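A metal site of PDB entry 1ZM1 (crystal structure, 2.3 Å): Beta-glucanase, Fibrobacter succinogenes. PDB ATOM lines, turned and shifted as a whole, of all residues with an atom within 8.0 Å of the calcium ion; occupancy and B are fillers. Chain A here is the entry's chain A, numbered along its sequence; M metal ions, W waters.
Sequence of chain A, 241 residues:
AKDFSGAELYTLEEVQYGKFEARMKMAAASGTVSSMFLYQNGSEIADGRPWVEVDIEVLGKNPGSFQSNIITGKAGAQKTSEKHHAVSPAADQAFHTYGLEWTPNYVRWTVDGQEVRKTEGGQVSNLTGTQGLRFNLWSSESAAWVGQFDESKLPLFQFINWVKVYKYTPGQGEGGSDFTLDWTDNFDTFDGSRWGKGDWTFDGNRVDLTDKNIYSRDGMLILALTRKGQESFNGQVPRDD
ND2 of Asn 161 is in hydrogen-bond range of OD1 of Asp 240, at 3.1 Å. The backbone carbonyl oxygen (O) of Arg 23 lies within hydrogen-bond range of the backbone NH (N) of Asn 161, 2.7 Å away.
O of Gly 219 binds the calcium ion. The calcium ion is bound by O of Asn 186 (2.4 Å). The calcium ion is bound by the backbone carbonyl oxygen (O) of Asn 161, 2.4 Å away. The calcium ion is bound by OD1 of Asn 161, 2.5 Å away. Water W3 is bound to the calcium ion, 2.7 Å away. Water W1 binds the calcium ion (2.7 Å). Water W2 binds the calcium ion. The calcium ion has seven donor atoms within binding distance.
Within 4 Å of the calcium ion: Asn 161, Asn 186 and Gly 219. The nearest printed residue that does not touch the calcium ion is Met 220 (4.5 Å).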
ATOM      1  N   ARG A  23       3.006 -27.298  12.024  1.00  0.00           N
ATOM      2  CA  ARG A  23       4.407 -27.278  11.614  1.00  0.00           C
ATOM      3  C   ARG A  23       5.180 -27.717  12.838  1.00  0.00           C
ATOM      4  O   ARG A  23       5.293 -26.974  13.828  1.00  0.00           O
ATOM      5  CB  ARG A  23       4.800 -25.846  11.206  1.00  0.00           C
ATOM      6  CG  ARG A  23       6.236 -25.691  10.741  1.00  0.00           C
ATOM      7  CD  ARG A  23       6.434 -26.290   9.365  1.00  0.00           C
ATOM      8  NE  ARG A  23       7.814 -26.207   8.924  1.00  0.00           N
ATOM      9  CZ  ARG A  23       8.313 -26.930   7.920  1.00  0.00           C
ATOM     10  NH1 ARG A  23       7.529 -27.772   7.269  1.00  0.00           N
ATOM     11  NH2 ARG A  23       9.595 -26.822   7.594  1.00  0.00           N
ATOM     12  N   ILE A 160       6.361 -27.356  18.135  1.00  0.00           N
ATOM     13  CA  ILE A 160       5.310 -26.997  17.202  1.00  0.00           C
ATOM     14  C   ILE A 160       5.486 -25.513  16.928  1.00  0.00           C
ATOM     15  O   ILE A 160       5.256 -24.684  17.815  1.00  0.00           O
ATOM     16  CB  ILE A 160       3.905 -27.265  17.784  1.00  0.00           C
ATOM     17  CG1 ILE A 160       3.783 -28.750  18.168  1.00  0.00           C
ATOM     18  CG2 ILE A 160       2.847 -26.887  16.780  1.00  0.00           C
ATOM     19  CD1 ILE A 160       2.449 -29.126  18.801  1.00  0.00           C
ATOM     20  N   ASN A 161       5.891 -25.173  15.712  1.00  0.00           N
ATOM     21  CA  ASN A 161       6.118 -23.790  15.341  1.00  0.00           C
ATOM     22  C   ASN A 161       4.801 -23.035  15.170  1.00  0.00           C
ATOM     23  O   ASN A 161       4.664 -21.896  15.605  1.00  0.00           O
ATOM     24  CB  ASN A 161       6.964 -23.727  14.061  1.00  0.00           C
ATOM     25  CG  ASN A 161       7.387 -22.311  13.696  1.00  0.00           C
ATOM     26  OD1 ASN A 161       7.561 -21.455  14.566  1.00  0.00           O
ATOM     27  ND2 ASN A 161       7.577 -22.056  12.409  1.00  0.00           N
ATOM     28  N   TRP A 162       3.838 -23.682  14.533  1.00  0.00           N
ATOM     29  CA  TRP A 162       2.525 -23.073  14.341  1.00  0.00           C
ATOM     30  C   TRP A 162       1.464 -24.092  13.995  1.00  0.00           C
ATOM     31  O   TRP A 162       1.756 -25.241  13.649  1.00  0.00           O
ATOM     32  CB  TRP A 162       2.554 -21.979  13.252  1.00  0.00           C
ATOM     33  CG  TRP A 162       3.106 -22.378  11.908  1.00  0.00           C
ATOM     34  CD1 TRP A 162       4.350 -22.081  11.423  1.00  0.00           C
ATOM     35  CD2 TRP A 162       2.446 -23.137  10.887  1.00  0.00           C
ATOM     36  NE1 TRP A 162       4.499 -22.601  10.146  1.00  0.00           N
ATOM     37  CE2 TRP A 162       3.344 -23.254   9.803  1.00  0.00           C
ATOM     38  CE3 TRP A 162       1.176 -23.715  10.776  1.00  0.00           C
ATOM     39  CZ2 TRP A 162       3.012 -23.938   8.616  1.00  0.00           C
ATOM     40  CZ3 TRP A 162       0.841 -24.408   9.592  1.00  0.00           C
ATOM     41  CH2 TRP A 162       1.761 -24.498   8.539  1.00  0.00           C
ATOM     42  N   VAL A 163       0.217 -23.647  14.112  1.00  0.00           N
ATOM     43  CA  VAL A 163      -0.928 -24.481  13.811  1.00  0.00           C
ATOM     44  C   VAL A 163      -1.956 -23.645  13.045  1.00  0.00           C
ATOM     45  O   VAL A 163      -2.202 -22.487  13.370  1.00  0.00           O
ATOM     46  CB  VAL A 163      -1.557 -25.027  15.103  1.00  0.00           C
ATOM     47  CG1 VAL A 163      -2.935 -25.570  14.805  1.00  0.00           C
ATOM     48  CG2 VAL A 163      -0.685 -26.133  15.671  1.00  0.00           C
ATOM     49  N   ASP A 185      -2.153 -20.001  14.810  1.00  0.00           N
ATOM     50  CA  ASP A 185      -1.481 -19.752  16.074  1.00  0.00           C
ATOM     51  C   ASP A 185      -0.007 -19.939  15.813  1.00  0.00           C
ATOM     52  O   ASP A 185       0.458 -21.044  15.511  1.00  0.00           O
ATOM     53  CB  ASP A 185      -1.942 -20.724  17.158  1.00  0.00           C
ATOM     54  CG  ASP A 185      -1.475 -20.307  18.544  1.00  0.00           C
ATOM     55  OD1 ASP A 185      -0.420 -19.647  18.636  1.00  0.00           O
ATOM     56  OD2 ASP A 185      -2.152 -20.632  19.544  1.00  0.00           O
ATOM     57  N   ASN A 186       0.740 -18.849  15.904  1.00  0.00           N
ATOM     58  CA  ASN A 186       2.165 -18.888  15.656  1.00  0.00           C
ATOM     59  C   ASN A 186       2.926 -19.172  16.943  1.00  0.00           C
ATOM     60  O   ASN A 186       4.155 -19.167  16.975  1.00  0.00           O
ATOM     61  CB  ASN A 186       2.594 -17.586  15.007  1.00  0.00           C
ATOM     62  CG  ASN A 186       2.048 -17.438  13.600  1.00  0.00           C
ATOM     63  OD1 ASN A 186       2.465 -18.151  12.689  1.00  0.00           O
ATOM     64  ND2 ASN A 186       1.079 -16.541  13.423  1.00  0.00           N
ATOM     65  N   PHE A 187       2.162 -19.434  17.995  1.00  0.00           N
ATOM     66  CA  PHE A 187       2.695 -19.749  19.311  1.00  0.00           C
ATOM     67  C   PHE A 187       3.757 -18.790  19.825  1.00  0.00           C
ATOM     68  O   PHE A 187       4.808 -19.226  20.300  1.00  0.00           O
ATOM     69  CB  PHE A 187       3.238 -21.187  19.331  1.00  0.00           C
ATOM     70  CG  PHE A 187       2.175 -22.237  19.162  1.00  0.00           C
ATOM     71  CD1 PHE A 187       2.083 -22.971  17.985  1.00  0.00           C
ATOM     72  CD2 PHE A 187       1.235 -22.463  20.174  1.00  0.00           C
ATOM     73  CE1 PHE A 187       1.075 -23.929  17.814  1.00  0.00           C
ATOM     74  CE2 PHE A 187       0.229 -23.406  20.012  1.00  0.00           C
ATOM     75  CZ  PHE A 187       0.145 -24.144  18.830  1.00  0.00           C
ATOM     76  N   ASP A 188       3.489 -17.489  19.740  1.00  0.00           N
ATOM     77  CA  ASP A 188       4.414 -16.501  20.260  1.00  0.00           C
ATOM     78  C   ASP A 188       4.167 -16.444  21.767  1.00  0.00           C
ATOM     79  O   ASP A 188       4.841 -15.729  22.513  1.00  0.00           O
ATOM     80  CB  ASP A 188       4.165 -15.127  19.623  1.00  0.00           C
ATOM     81  CG  ASP A 188       4.630 -15.068  18.181  1.00  0.00           C
ATOM     82  OD1 ASP A 188       5.757 -15.535  17.893  1.00  0.00           O
ATOM     83  OD2 ASP A 188       3.870 -14.556  17.331  1.00  0.00           O
ATOM     84  N   THR A 189       3.179 -17.234  22.188  1.00  0.00           N
ATOM     85  CA  THR A 189       2.791 -17.384  23.588  1.00  0.00           C
ATOM     86  C   THR A 189       1.706 -18.457  23.659  1.00  0.00           C
ATOM     87  O   THR A 189       1.206 -18.903  22.632  1.00  0.00           O
ATOM     88  CB  THR A 189       2.205 -16.091  24.171  1.00  0.00           C
ATOM     89  OG1 THR A 189       1.836 -16.337  25.546  1.00  0.00           O
ATOM     90  CG2 THR A 189       0.975 -15.646  23.378  1.00  0.00           C
ATOM     91  N   ARG A 217       8.488 -20.826  23.732  1.00  0.00           N
ATOM     92  CA  ARG A 217       9.835 -20.265  23.729  1.00  0.00           C
ATOM     93  C   ARG A 217      10.243 -19.972  22.308  1.00  0.00           C
ATOM     94  O   ARG A 217      10.155 -20.829  21.427  1.00  0.00           O
ATOM     95  CB  ARG A 217      10.841 -21.237  24.357  1.00  0.00           C
ATOM     96  CG  ARG A 217      11.401 -20.770  25.696  1.00  0.00           C
ATOM     97  CD  ARG A 217      12.595 -21.593  26.099  1.00  0.00           C
ATOM     98  NE  ARG A 217      13.128 -21.229  27.409  1.00  0.00           N
ATOM     99  CZ  ARG A 217      14.227 -21.774  27.940  1.00  0.00           C
ATOM    100  NH1 ARG A 217      14.902 -22.686  27.255  1.00  0.00           N
ATOM    101  NH2 ARG A 217      14.647 -21.399  29.144  1.00  0.00           N
ATOM    102  N   ASP A 218      10.686 -18.749  22.078  1.00  0.00           N
ATOM    103  CA  ASP A 218      11.141 -18.339  20.768  1.00  0.00           C
ATOM    104  C   ASP A 218      10.143 -18.709  19.674  1.00  0.00           C
ATOM    105  O   ASP A 218      10.487 -19.365  18.696  1.00  0.00           O
ATOM    106  CB  ASP A 218      12.499 -18.977  20.463  1.00  0.00           C
ATOM    107  CG  ASP A 218      13.550 -18.623  21.509  1.00  0.00           C
ATOM    108  OD1 ASP A 218      13.841 -17.418  21.671  1.00  0.00           O
ATOM    109  OD2 ASP A 218      14.073 -19.544  22.163  1.00  0.00           O
ATOM    110  N   GLY A 219       8.900 -18.278  19.876  1.00  0.00           N
ATOM    111  CA  GLY A 219       7.851 -18.526  18.901  1.00  0.00           C
ATOM    112  C   GLY A 219       7.424 -19.968  18.731  1.00  0.00           C
ATOM    113  O   GLY A 219       6.833 -20.319  17.718  1.00  0.00           O
ATOM    114  N   MET A 220       7.712 -20.801  19.710  1.00  0.00           N
ATOM    115  CA  MET A 220       7.304 -22.189  19.581  1.00  0.00           C
ATOM    116  C   MET A 220       6.750 -22.820  20.843  1.00  0.00           C
ATOM    117  O   MET A 220       7.186 -22.513  21.947  1.00  0.00           O
ATOM    118  CB  MET A 220       8.468 -23.033  19.060  1.00  0.00           C
ATOM    119  CG  MET A 220       8.697 -22.845  17.582  1.00  0.00           C
ATOM    120  SD  MET A 220       9.651 -24.282  16.772  1.00  0.00           S
ATOM    121  CE  MET A 220      11.199 -23.308  16.154  1.00  0.00           C
ATOM    122  N   LEU A 221       5.757 -23.689  20.651  1.00  0.00           N
ATOM    123  CA  LEU A 221       5.153 -24.390  21.773  1.00  0.00           C
ATOM    124  C   LEU A 221       5.948 -25.689  21.892  1.00  0.00           C
ATOM    125  O   LEU A 221       6.221 -26.351  20.891  1.00  0.00           O
ATOM    126  CB  LEU A 221       3.676 -24.684  21.498  1.00  0.00           C
ATOM    127  CG  LEU A 221       2.775 -25.048  22.686  1.00  0.00           C
ATOM    128  CD1 LEU A 221       3.162 -26.395  23.283  1.00  0.00           C
ATOM    129  CD2 LEU A 221       2.863 -23.945  23.730  1.00  0.00           C
ATOM    130  N   ASP A 240      13.400 -23.297  12.414  1.00  0.00           N
ATOM    131  CA  ASP A 240      12.604 -23.824  11.310  1.00  0.00           C
ATOM    132  C   ASP A 240      12.904 -22.930  10.106  1.00  0.00           C
ATOM    133  O   ASP A 240      12.114 -22.043   9.780  1.00  0.00           O
ATOM    134  CB  ASP A 240      11.116 -23.777  11.662  1.00  0.00           C
ATOM    135  CG  ASP A 240      10.242 -24.383  10.575  1.00  0.00           C
ATOM    136  OD1 ASP A 240       9.008 -24.262  10.689  1.00  0.00           O
ATOM    137  OD2 ASP A 240      10.794 -24.968   9.625  1.00  0.00           O
HETATM  138 CA    CA M   1       6.003 -19.877  15.610  1.00  0.00          CA
HETATM  139  O   HOH W   1       8.266 -18.752  14.567  1.00  0.00           O
HETATM  140  O   HOH W   2       6.560 -17.166  15.345  1.00  0.00           O
HETATM  141  O   HOH W   3       4.931 -19.232  13.214  1.00  0.00           O
